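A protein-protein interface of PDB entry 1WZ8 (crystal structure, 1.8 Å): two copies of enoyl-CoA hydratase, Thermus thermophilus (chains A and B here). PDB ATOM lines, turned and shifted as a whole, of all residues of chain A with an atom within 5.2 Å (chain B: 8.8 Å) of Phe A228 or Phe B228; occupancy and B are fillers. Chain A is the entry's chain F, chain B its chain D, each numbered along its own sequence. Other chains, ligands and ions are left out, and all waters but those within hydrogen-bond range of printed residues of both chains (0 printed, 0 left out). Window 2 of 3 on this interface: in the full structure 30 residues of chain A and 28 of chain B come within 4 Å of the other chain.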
ATOM      1  N   LEU A 154      11.584  34.730   6.448  1.00  0.00           N
ATOM      2  CA  LEU A 154      12.422  33.697   7.043  1.00  0.00           C
ATOM      3  C   LEU A 154      13.760  34.264   7.491  1.00  0.00           C
ATOM      4  O   LEU A 154      14.271  33.907   8.551  1.00  0.00           O
ATOM      5  CB  LEU A 154      12.704  32.563   6.051  1.00  0.00           C
ATOM      6  CG  LEU A 154      13.594  31.431   6.600  1.00  0.00           C
ATOM      7  CD1 LEU A 154      12.796  30.585   7.580  1.00  0.00           C
ATOM      8  CD2 LEU A 154      14.120  30.554   5.454  1.00  0.00           C
ATOM      9  N   LEU A 158      16.100  37.824  11.800  1.00  0.00           N
ATOM     10  CA  LEU A 158      17.330  37.386  12.463  1.00  0.00           C
ATOM     11  C   LEU A 158      18.584  37.975  11.829  1.00  0.00           C
ATOM     12  O   LEU A 158      19.699  37.620  12.208  1.00  0.00           O
ATOM     13  CB  LEU A 158      17.438  35.856  12.467  1.00  0.00           C
ATOM     14  CG  LEU A 158      16.469  35.115  13.392  1.00  0.00           C
ATOM     15  CD1 LEU A 158      16.686  33.618  13.256  1.00  0.00           C
ATOM     16  CD2 LEU A 158      16.686  35.563  14.835  1.00  0.00           C
ATOM     17  N   TRP A 224      18.030  27.668  13.608  1.00  0.00           N
ATOM     18  CA  TRP A 224      17.392  28.909  14.031  1.00  0.00           C
ATOM     19  C   TRP A 224      16.398  29.292  12.947  1.00  0.00           C
ATOM     20  O   TRP A 224      15.261  29.669  13.228  1.00  0.00           O
ATOM     21  CB  TRP A 224      18.421  30.026  14.198  1.00  0.00           C
ATOM     22  CG  TRP A 224      19.113  29.987  15.513  1.00  0.00           C
ATOM     23  CD1 TRP A 224      20.139  29.165  15.881  1.00  0.00           C
ATOM     24  CD2 TRP A 224      18.779  30.759  16.670  1.00  0.00           C
ATOM     25  NE1 TRP A 224      20.462  29.376  17.201  1.00  0.00           N
ATOM     26  CE2 TRP A 224      19.642  30.349  17.708  1.00  0.00           C
ATOM     27  CE3 TRP A 224      17.831  31.758  16.930  1.00  0.00           C
ATOM     28  CZ2 TRP A 224      19.586  30.904  18.994  1.00  0.00           C
ATOM     29  CZ3 TRP A 224      17.775  32.311  18.207  1.00  0.00           C
ATOM     30  CH2 TRP A 224      18.649  31.880  19.223  1.00  0.00           C
ATOM     31  N   TYR A 225      16.833  29.188  11.695  1.00  0.00           N
ATOM     32  CA  TYR A 225      15.953  29.511  10.585  1.00  0.00           C
ATOM     33  C   TYR A 225      14.845  28.471  10.444  1.00  0.00           C
ATOM     34  O   TYR A 225      13.677  28.818  10.240  1.00  0.00           O
ATOM     35  CB  TYR A 225      16.731  29.581   9.272  1.00  0.00           C
ATOM     36  CG  TYR A 225      17.568  30.824   9.080  1.00  0.00           C
ATOM     37  CD1 TYR A 225      17.058  32.090   9.375  1.00  0.00           C
ATOM     38  CD2 TYR A 225      18.838  30.742   8.511  1.00  0.00           C
ATOM     39  CE1 TYR A 225      17.787  33.240   9.104  1.00  0.00           C
ATOM     40  CE2 TYR A 225      19.572  31.884   8.231  1.00  0.00           C
ATOM     41  CZ  TYR A 225      19.042  33.129   8.525  1.00  0.00           C
ATOM     42  OH  TYR A 225      19.743  34.259   8.185  1.00  0.00           O
ATOM     43  N   ARG A 226      15.211  27.194  10.535  1.00  0.00           N
ATOM     44  CA  ARG A 226      14.230  26.120  10.408  1.00  0.00           C
ATOM     45  C   ARG A 226      13.097  26.211  11.429  1.00  0.00           C
ATOM     46  O   ARG A 226      11.981  25.764  11.160  1.00  0.00           O
ATOM     47  CB  ARG A 226      14.910  24.749  10.525  1.00  0.00           C
ATOM     48  CG  ARG A 226      16.019  24.505   9.496  1.00  0.00           C
ATOM     49  CD  ARG A 226      16.449  23.038   9.494  1.00  0.00           C
ATOM     50  NE  ARG A 226      17.587  22.790   8.609  1.00  0.00           N
ATOM     51  CZ  ARG A 226      18.859  22.790   9.004  1.00  0.00           C
ATOM     52  NH1 ARG A 226      19.165  23.020  10.275  1.00  0.00           N
ATOM     53  NH2 ARG A 226      19.830  22.564   8.125  1.00  0.00           N
ATOM     54  N   SER A 227      13.369  26.787  12.599  1.00  0.00           N
ATOM     55  CA  SER A 227      12.327  26.909  13.621  1.00  0.00           C
ATOM     56  C   SER A 227      11.213  27.849  13.172  1.00  0.00           C
ATOM     57  O   SER A 227      10.102  27.820  13.710  1.00  0.00           O
ATOM     58  CB  SER A 227      12.916  27.409  14.942  1.00  0.00           C
ATOM     59  OG  SER A 227      13.633  26.376  15.589  1.00  0.00           O
ATOM     60  N   PHE A 228      11.515  28.676  12.178  1.00  0.00           N
ATOM     61  CA  PHE A 228      10.549  29.621  11.652  1.00  0.00           C
ATOM     62  C   PHE A 228      10.117  29.275  10.230  1.00  0.00           C
ATOM     63  O   PHE A 228       9.649  30.136   9.488  1.00  0.00           O
ATOM     64  CB  PHE A 228      11.134  31.032  11.719  1.00  0.00           C
ATOM     65  CG  PHE A 228      11.332  31.522  13.125  1.00  0.00           C
ATOM     66  CD1 PHE A 228      10.314  32.201  13.788  1.00  0.00           C
ATOM     67  CD2 PHE A 228      12.514  31.252  13.808  1.00  0.00           C
ATOM     68  CE1 PHE A 228      10.468  32.599  15.111  1.00  0.00           C
ATOM     69  CE2 PHE A 228      12.678  31.647  15.135  1.00  0.00           C
ATOM     70  CZ  PHE A 228      11.653  32.321  15.787  1.00  0.00           C
ATOM     71  N   LEU A 229      10.266  28.012   9.846  1.00  0.00           N
ATOM     72  CA  LEU A 229       9.859  27.607   8.502  1.00  0.00           C
ATOM     73  C   LEU A 229       8.368  27.819   8.256  1.00  0.00           C
ATOM     74  O   LEU A 229       7.962  28.265   7.183  1.00  0.00           O
ATOM     75  CB  LEU A 229      10.245  26.153   8.232  1.00  0.00           C
ATOM     76  CG  LEU A 229      11.656  25.980   7.659  1.00  0.00           C
ATOM     77  CD1 LEU A 229      11.958  24.494   7.425  1.00  0.00           C
ATOM     78  CD2 LEU A 229      11.758  26.750   6.343  1.00  0.00           C
ATOM     79  N   PRO A 230       7.521  27.493   9.242  1.00  0.00           N
ATOM     80  CA  PRO A 230       6.092  27.708   9.002  1.00  0.00           C
ATOM     81  C   PRO A 230       5.816  29.199   8.758  1.00  0.00           C
ATOM     82  O   PRO A 230       4.972  29.567   7.941  1.00  0.00           O
ATOM     83  CB  PRO A 230       5.455  27.201  10.290  1.00  0.00           C
ATOM     84  CG  PRO A 230       6.376  26.094  10.695  1.00  0.00           C
ATOM     85  CD  PRO A 230       7.738  26.702  10.467  1.00  0.00           C
ATOM     86  N   HIS A 231       6.535  30.056   9.475  1.00  0.00           N
ATOM     87  CA  HIS A 231       6.362  31.497   9.322  1.00  0.00           C
ATOM     88  C   HIS A 231       6.662  31.880   7.880  1.00  0.00           C
ATOM     89  O   HIS A 231       5.935  32.653   7.255  1.00  0.00           O
ATOM     90  CB  HIS A 231       7.327  32.253  10.230  1.00  0.00           C
ATOM     91  CG  HIS A 231       7.112  32.002  11.688  1.00  0.00           C
ATOM     92  ND1 HIS A 231       7.139  30.738  12.238  1.00  0.00           N
ATOM     93  CD2 HIS A 231       6.887  32.856  12.712  1.00  0.00           C
ATOM     94  CE1 HIS A 231       6.943  30.826  13.542  1.00  0.00           C
ATOM     95  NE2 HIS A 231       6.787  32.101  13.855  1.00  0.00           N
ATOM     96  N   PHE A 232       7.753  31.325   7.370  1.00  0.00           N
ATOM     97  CA  PHE A 232       8.199  31.588   6.009  1.00  0.00           C
ATOM     98  C   PHE A 232       7.220  31.078   4.962  1.00  0.00           C
ATOM     99  O   PHE A 232       6.823  31.818   4.060  1.00  0.00           O
ATOM    100  CB  PHE A 232       9.574  30.951   5.781  1.00  0.00           C
ATOM    101  CG  PHE A 232      10.010  30.957   4.348  1.00  0.00           C
ATOM    102  CD1 PHE A 232       9.901  32.116   3.581  1.00  0.00           C
ATOM    103  CD2 PHE A 232      10.521  29.807   3.760  1.00  0.00           C
ATOM    104  CE1 PHE A 232      10.294  32.129   2.249  1.00  0.00           C
ATOM    105  CE2 PHE A 232      10.921  29.806   2.421  1.00  0.00           C
ATOM    106  CZ  PHE A 232      10.806  30.970   1.661  1.00  0.00           C
ATOM    107  N   LEU B  98      24.478  27.856  30.988  1.00  0.00           N
ATOM    108  CA  LEU B  98      23.196  27.901  31.681  1.00  0.00           C
ATOM    109  C   LEU B  98      23.303  28.363  33.126  1.00  0.00           C
ATOM    110  O   LEU B  98      22.355  28.932  33.668  1.00  0.00           O
ATOM    111  CB  LEU B  98      22.517  26.534  31.637  1.00  0.00           C
ATOM    112  CG  LEU B  98      22.139  26.011  30.258  1.00  0.00           C
ATOM    113  CD1 LEU B  98      21.099  24.910  30.437  1.00  0.00           C
ATOM    114  CD2 LEU B  98      21.586  27.136  29.395  1.00  0.00           C
ATOM    115  N   HIS B 151      28.679  27.435  22.963  1.00  0.00           N
ATOM    116  CA  HIS B 151      27.893  28.630  23.294  1.00  0.00           C
ATOM    117  C   HIS B 151      27.354  29.396  22.093  1.00  0.00           C
ATOM    118  O   HIS B 151      26.250  29.922  22.134  1.00  0.00           O
ATOM    119  CB  HIS B 151      28.701  29.623  24.146  1.00  0.00           C
ATOM    120  CG  HIS B 151      29.567  30.539  23.341  1.00  0.00           C
ATOM    121  ND1 HIS B 151      30.770  30.142  22.803  1.00  0.00           N
ATOM    122  CD2 HIS B 151      29.378  31.820  22.937  1.00  0.00           C
ATOM    123  CE1 HIS B 151      31.286  31.134  22.098  1.00  0.00           C
ATOM    124  NE2 HIS B 151      30.460  32.163  22.163  1.00  0.00           N
ATOM    125  N   VAL B 153      25.910  28.777  19.231  1.00  0.00           N
ATOM    126  CA  VAL B 153      24.597  28.513  18.658  1.00  0.00           C
ATOM    127  C   VAL B 153      23.466  28.912  19.593  1.00  0.00           C
ATOM    128  O   VAL B 153      22.331  29.078  19.156  1.00  0.00           O
ATOM    129  CB  VAL B 153      24.463  27.025  18.250  1.00  0.00           C
ATOM    130  CG1 VAL B 153      23.045  26.725  17.773  1.00  0.00           C
ATOM    131  CG2 VAL B 153      25.455  26.724  17.146  1.00  0.00           C
ATOM    132  N   LEU B 154      23.769  29.077  20.877  1.00  0.00           N
ATOM    133  CA  LEU B 154      22.733  29.490  21.804  1.00  0.00           C
ATOM    134  C   LEU B 154      22.651  31.011  21.888  1.00  0.00           C
ATOM    135  O   LEU B 154      21.560  31.571  21.883  1.00  0.00           O
ATOM    136  CB  LEU B 154      22.992  28.946  23.216  1.00  0.00           C
ATOM    137  CG  LEU B 154      21.986  29.452  24.263  1.00  0.00           C
ATOM    138  CD1 LEU B 154      20.615  28.860  23.965  1.00  0.00           C
ATOM    139  CD2 LEU B 154      22.426  29.066  25.669  1.00  0.00           C
ATOM    140  N   LEU B 155      23.808  31.672  21.906  1.00  0.00           N
ATOM    141  CA  LEU B 155      23.860  33.121  22.092  1.00  0.00           C
ATOM    142  C   LEU B 155      24.081  34.071  20.906  1.00  0.00           C
ATOM    143  O   LEU B 155      23.449  35.124  20.849  1.00  0.00           O
ATOM    144  CB  LEU B 155      24.916  33.439  23.158  1.00  0.00           C
ATOM    145  CG  LEU B 155      24.961  32.571  24.426  1.00  0.00           C
ATOM    146  CD1 LEU B 155      26.182  32.957  25.270  1.00  0.00           C
ATOM    147  CD2 LEU B 155      23.679  32.738  25.223  1.00  0.00           C
ATOM    148  N   PRO B 157      23.185  34.275  17.536  1.00  0.00           N
ATOM    149  CA  PRO B 157      22.088  34.758  16.689  1.00  0.00           C
ATOM    150  C   PRO B 157      21.282  35.926  17.266  1.00  0.00           C
ATOM    151  O   PRO B 157      21.012  36.898  16.563  1.00  0.00           O
ATOM    152  CB  PRO B 157      21.240  33.502  16.477  1.00  0.00           C
ATOM    153  CG  PRO B 157      22.275  32.415  16.469  1.00  0.00           C
ATOM    154  CD  PRO B 157      23.145  32.805  17.654  1.00  0.00           C
ATOM    155  N   LEU B 158      20.898  35.839  18.537  1.00  0.00           N
ATOM    156  CA  LEU B 158      20.125  36.916  19.153  1.00  0.00           C
ATOM    157  C   LEU B 158      20.989  38.084  19.629  1.00  0.00           C
ATOM    158  O   LEU B 158      20.481  39.026  20.245  1.00  0.00           O
ATOM    159  CB  LEU B 158      19.293  36.387  20.325  1.00  0.00           C
ATOM    160  CG  LEU B 158      18.126  35.462  19.969  1.00  0.00           C
ATOM    161  CD1 LEU B 158      17.412  35.053  21.247  1.00  0.00           C
ATOM    162  CD2 LEU B 158      17.164  36.166  19.024  1.00  0.00           C
ATOM    163  N   MET B 162      22.322  36.462  12.238  1.00  0.00           N
ATOM    164  CA  MET B 162      22.898  35.290  11.580  1.00  0.00           C
ATOM    165  C   MET B 162      24.028  35.539  10.590  1.00  0.00           C
ATOM    166  O   MET B 162      24.904  34.693  10.445  1.00  0.00           O
ATOM    167  CB  MET B 162      21.801  34.494  10.878  1.00  0.00           C
ATOM    168  CG  MET B 162      22.233  33.088  10.481  1.00  0.00           C
ATOM    169  SD  MET B 162      22.750  32.149  11.946  1.00  0.00           S
ATOM    170  CE  MET B 162      21.177  31.912  12.749  1.00  0.00           C
ATOM    171  N   ASN B 222      15.719  35.892  29.646  1.00  0.00           N
ATOM    172  CA  ASN B 222      16.464  34.678  29.345  1.00  0.00           C
ATOM    173  C   ASN B 222      15.633  33.545  28.765  1.00  0.00           C
ATOM    174  O   ASN B 222      16.188  32.575  28.246  1.00  0.00           O
ATOM    175  CB  ASN B 222      17.260  34.220  30.573  1.00  0.00           C
ATOM    176  CG  ASN B 222      18.540  35.019  30.750  1.00  0.00           C
ATOM    177  OD1 ASN B 222      18.965  35.725  29.835  1.00  0.00           O
ATOM    178  ND2 ASN B 222      19.167  34.904  31.916  1.00  0.00           N
ATOM    179  N   HIS B 223      14.311  33.660  28.830  1.00  0.00           N
ATOM    180  CA  HIS B 223      13.466  32.625  28.239  1.00  0.00           C
ATOM    181  C   HIS B 223      13.661  32.631  26.723  1.00  0.00           C
ATOM    182  O   HIS B 223      13.353  31.648  26.045  1.00  0.00           O
ATOM    183  CB  HIS B 223      11.993  32.855  28.571  1.00  0.00           C
ATOM    184  CG  HIS B 223      11.530  32.126  29.795  1.00  0.00           C
ATOM    185  ND1 HIS B 223      11.776  30.785  29.999  1.00  0.00           N
ATOM    186  CD2 HIS B 223      10.814  32.544  30.866  1.00  0.00           C
ATOM    187  CE1 HIS B 223      11.230  30.409  31.142  1.00  0.00           C
ATOM    188  NE2 HIS B 223      10.640  31.457  31.688  1.00  0.00           N
ATOM    189  N   TRP B 224      14.152  33.750  26.188  1.00  0.00           N
ATOM    190  CA  TRP B 224      14.411  33.838  24.750  1.00  0.00           C
ATOM    191  C   TRP B 224      15.521  32.848  24.419  1.00  0.00           C
ATOM    192  O   TRP B 224      15.485  32.171  23.384  1.00  0.00           O
ATOM    193  CB  TRP B 224      14.852  35.249  24.350  1.00  0.00           C
ATOM    194  CG  TRP B 224      13.709  36.182  24.121  1.00  0.00           C
ATOM    195  CD1 TRP B 224      12.952  36.804  25.070  1.00  0.00           C
ATOM    196  CD2 TRP B 224      13.154  36.557  22.852  1.00  0.00           C
ATOM    197  NE1 TRP B 224      11.955  37.541  24.470  1.00  0.00           N
ATOM    198  CE2 TRP B 224      12.059  37.406  23.109  1.00  0.00           C
ATOM    199  CE3 TRP B 224      13.476  36.252  21.522  1.00  0.00           C
ATOM    200  CZ2 TRP B 224      11.280  37.961  22.085  1.00  0.00           C
ATOM    201  CZ3 TRP B 224      12.703  36.801  20.501  1.00  0.00           C
ATOM    202  CH2 TRP B 224      11.617  37.649  20.791  1.00  0.00           C
ATOM    203  N   TYR B 225      16.519  32.777  25.294  1.00  0.00           N
ATOM    204  CA  TYR B 225      17.620  31.842  25.092  1.00  0.00           C
ATOM    205  C   TYR B 225      17.130  30.430  25.400  1.00  0.00           C
ATOM    206  O   TYR B 225      17.455  29.480  24.691  1.00  0.00           O
ATOM    207  CB  TYR B 225      18.804  32.159  26.015  1.00  0.00           C
ATOM    208  CG  TYR B 225      19.669  33.343  25.613  1.00  0.00           C
ATOM    209  CD1 TYR B 225      20.126  33.499  24.303  1.00  0.00           C
ATOM    210  CD2 TYR B 225      20.085  34.272  26.568  1.00  0.00           C
ATOM    211  CE1 TYR B 225      20.986  34.556  23.957  1.00  0.00           C
ATOM    212  CE2 TYR B 225      20.933  35.321  26.236  1.00  0.00           C
ATOM    213  CZ  TYR B 225      21.382  35.459  24.936  1.00  0.00           C
ATOM    214  OH  TYR B 225      22.239  36.492  24.629  1.00  0.00           O
ATOM    215  N   ARG B 226      16.341  30.290  26.461  1.00  0.00           N
ATOM    216  CA  ARG B 226      15.852  28.971  26.844  1.00  0.00           C
ATOM    217  C   ARG B 226      15.020  28.288  25.763  1.00  0.00           C
ATOM    218  O   ARG B 226      15.003  27.060  25.686  1.00  0.00           O
ATOM    219  CB  ARG B 226      15.044  29.045  28.147  1.00  0.00           C
ATOM    220  CG  ARG B 226      15.852  29.492  29.347  1.00  0.00           C
ATOM    221  CD  ARG B 226      15.047  29.345  30.642  1.00  0.00           C
ATOM    222  NE  ARG B 226      15.737  29.958  31.769  1.00  0.00           N
ATOM    223  CZ  ARG B 226      15.455  31.164  32.250  1.00  0.00           C
ATOM    224  NH1 ARG B 226      14.484  31.891  31.708  1.00  0.00           N
ATOM    225  NH2 ARG B 226      16.163  31.654  33.259  1.00  0.00           N
ATOM    226  N   SER B 227      14.336  29.070  24.931  1.00  0.00           N
ATOM    227  CA  SER B 227      13.516  28.496  23.866  1.00  0.00           C
ATOM    228  C   SER B 227      14.387  27.812  22.821  1.00  0.00           C
ATOM    229  O   SER B 227      13.905  26.995  22.038  1.00  0.00           O
ATOM    230  CB  SER B 227      12.675  29.580  23.179  1.00  0.00           C
ATOM    231  OG  SER B 227      11.675  30.087  24.047  1.00  0.00           O
ATOM    232  N   PHE B 228      15.672  28.152  22.815  1.00  0.00           N
ATOM    233  CA  PHE B 228      16.601  27.579  21.846  1.00  0.00           C
ATOM    234  C   PHE B 228      17.632  26.640  22.466  1.00  0.00           C
ATOM    235  O   PHE B 228      18.683  26.380  21.874  1.00  0.00           O
ATOM    236  CB  PHE B 228      17.297  28.708  21.085  1.00  0.00           C
ATOM    237  CG  PHE B 228      16.377  29.474  20.179  1.00  0.00           C
ATOM    238  CD1 PHE B 228      16.142  29.034  18.880  1.00  0.00           C
ATOM    239  CD2 PHE B 228      15.695  30.601  20.643  1.00  0.00           C
ATOM    240  CE1 PHE B 228      15.253  29.703  18.052  1.00  0.00           C
ATOM    241  CE2 PHE B 228      14.801  31.280  19.820  1.00  0.00           C
ATOM    242  CZ  PHE B 228      14.574  30.826  18.520  1.00  0.00           C
ATOM    243  N   LEU B 229      17.329  26.123  23.655  1.00  0.00           N
ATOM    244  CA  LEU B 229      18.239  25.205  24.323  1.00  0.00           C
ATOM    245  C   LEU B 229      18.537  23.946  23.513  1.00  0.00           C
ATOM    246  O   LEU B 229      19.677  23.488  23.493  1.00  0.00           O
ATOM    247  CB  LEU B 229      17.706  24.812  25.703  1.00  0.00           C
ATOM    248  CG  LEU B 229      18.142  25.730  26.844  1.00  0.00           C
ATOM    249  CD1 LEU B 229      17.606  25.196  28.174  1.00  0.00           C
ATOM    250  CD2 LEU B 229      19.668  25.789  26.880  1.00  0.00           C
ATOM    251  N   PRO B 230      17.522  23.358  22.853  1.00  0.00           N
ATOM    252  CA  PRO B 230      17.786  22.151  22.059  1.00  0.00           C
ATOM    253  C   PRO B 230      18.782  22.456  20.927  1.00  0.00           C
ATOM    254  O   PRO B 230      19.665  21.647  20.614  1.00  0.00           O
ATOM    255  CB  PRO B 230      16.406  21.776  21.517  1.00  0.00           C
ATOM    256  CG  PRO B 230      15.466  22.319  22.558  1.00  0.00           C
ATOM    257  CD  PRO B 230      16.076  23.637  22.936  1.00  0.00           C
ATOM    258  N   HIS B 231      18.627  23.631  20.318  1.00  0.00           N
ATOM    259  CA  HIS B 231      19.510  24.068  19.242  1.00  0.00           C
ATOM    260  C   HIS B 231      20.943  24.059  19.771  1.00  0.00           C
ATOM    261  O   HIS B 231      21.866  23.571  19.121  1.00  0.00           O
ATOM    262  CB  HIS B 231      19.143  25.495  18.802  1.00  0.00           C
ATOM    263  CG  HIS B 231      17.752  25.633  18.258  1.00  0.00           C
ATOM    264  ND1 HIS B 231      16.631  25.242  18.958  1.00  0.00           N
ATOM    265  CD2 HIS B 231      17.304  26.120  17.076  1.00  0.00           C
ATOM    266  CE1 HIS B 231      15.554  25.480  18.230  1.00  0.00           C
ATOM    267  NE2 HIS B 231      15.936  26.012  17.082  1.00  0.00           N
ATOM    268  N   PHE B 232      21.112  24.611  20.967  1.00  0.00           N
ATOM    269  CA  PHE B 232      22.417  24.700  21.617  1.00  0.00           C
ATOM    270  C   PHE B 232      23.000  23.341  21.996  1.00  0.00           C
ATOM    271  O   PHE B 232      24.136  23.023  21.656  1.00  0.00           O
ATOM    272  CB  PHE B 232      22.296  25.583  22.866  1.00  0.00           C
ATOM    273  CG  PHE B 232      23.502  25.537  23.777  1.00  0.00           C
ATOM    274  CD1 PHE B 232      24.783  25.801  23.286  1.00  0.00           C
ATOM    275  CD2 PHE B 232      23.346  25.268  25.137  1.00  0.00           C
ATOM    276  CE1 PHE B 232      25.892  25.801  24.137  1.00  0.00           C
ATOM    277  CE2 PHE B 232      24.449  25.265  26.000  1.00  0.00           C
ATOM    278  CZ  PHE B 232      25.725  25.535  25.498  1.00  0.00           C
ATOM    279  N   GLU B 233      22.219  22.537  22.700  1.00  0.00           N
ATOM    280  CA  GLU B 233      22.713  21.240  23.123  1.00  0.00           C
ATOM    281  C   GLU B 233      23.050  20.330  21.953  1.00  0.00           C
ATOM    282  O   GLU B 233      23.928  19.476  22.064  1.00  0.00           O
ATOM    283  CB  GLU B 233      21.709  20.600  24.076  1.00  0.00           C
ATOM    284  CG  GLU B 233      21.628  21.382  25.390  1.00  0.00           C
ATOM    285  CD  GLU B 233      20.642  20.803  26.372  1.00  0.00           C
ATOM    286  OE1 GLU B 233      20.254  19.634  26.201  1.00  0.00           O
ATOM    287  OE2 GLU B 233      20.267  21.520  27.326  1.00  0.00           O
ATOM    288  N   LEU B 234      22.364  20.522  20.830  1.00  0.00           N
ATOM    289  CA  LEU B 234      22.647  19.730  19.636  1.00  0.00           C
ATOM    290  C   LEU B 234      24.018  20.145  19.102  1.00  0.00           C
ATOM    291  O   LEU B 234      24.840  19.298  18.749  1.00  0.00           O
ATOM    292  CB  LEU B 234      21.588  19.974  18.553  1.00  0.00           C
ATOM    293  CG  LEU B 234      21.930  19.417  17.163  1.00  0.00           C
ATOM    294  CD1 LEU B 234      22.145  17.904  17.236  1.00  0.00           C
ATOM    295  CD2 LEU B 234      20.813  19.752  16.188  1.00  0.00           C
ATOM    296  N   SER B 235      24.263  21.451  19.039  1.00  0.00           N
ATOM    297  CA  SER B 235      25.548  21.934  18.548  1.00  0.00           C
ATOM    298  C   SER B 235      26.659  21.432  19.462  1.00  0.00           C
ATOM    299  O   SER B 235      27.757  21.119  19.001  1.00  0.00           O
ATOM    300  CB  SER B 235      25.576  23.467  18.484  1.00  0.00           C
ATOM    301  OG  SER B 235      25.669  24.050  19.774  1.00  0.00           O
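N of Met B162 is in hydrogen-bond range of O of Leu A158, at 2.9 Å.
OG of Ser A227 is in hydrogen-bond range of NE2 of His B231.
The indole nitrogen (NE1) of Trp A224 is in hydrogen-bond range of the backbone carbonyl oxygen (O) of Val B153, 2.7 Å away.
Leu B154 touches Trp A224 (O to CZ2, 3.6 Å).
CE2 of Trp A224 touches CG of Pro B157 (3.6 Å).
Trp A224 touches Leu B158 (CZ3 to CG, 3.6 Å).
Trp A224 touches Met B162.
Trp A224 touches Phe B228.
Trp A224 touches His B231.
Tyr A225 touches Met B162 (OH to CB, 3.4 Å).
CE2 of Phe A228 touches CZ of Phe B228, 3.97 Å away.
Of chain B, only Phe B228 (3.97 Å) comes within 4 Å of Phe A228.
Phe B228 touches two residues of chain A.
Of chain B, only His B231 (2.8 Å) comes within 4 Å of Ser A227.
Of the printed residues of chain A, Leu B154 touches Trp A224 (3.6 Å).
Of the printed residues of chain A, Leu B158 touches Trp A224 (3.6 Å).
Trp B224 touches none of the printed residues of chain A.
His B223 touches none of the printed residues of chain A.
The nearest residue of chain B that does not touch Phe A228 is Trp B224 (6.6 Å).
The nearest residue of chain A that does not touch Phe B228 is Ser A227 (4.4 Å).
The nearest printed residue of chain A that does not touch Val B153 is Tyr A225 (9.0 Å).
Of the 22 printed residues of chain B, 7 touch a printed residue of chain A.
Printed residues of chain A that touch a printed residue of chain B: Leu A158, Trp A224, Tyr A225, Ser A227 and Phe A228.
Among the printed residues, 11 pairs touch across the chains.
Among the printed residues, no Asp or Glu carboxylate lies within 4 Å of a Lys or Arg side-chain nitrogen of the other chain.
Trp A224 touches Leu B158, but with the chains exchanged Leu A158 does not touch Trp B224 (7.0 Å).
Trp A224 touches His B231, but with the chains exchanged His A231 does not touch Trp B224 (10.1 Å).
Ser A227 touches His B231, but with the chains exchanged His A231 does not touch Ser B227 (11.3 Å).
Phe A228 touches its own counterpart, Phe B228.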
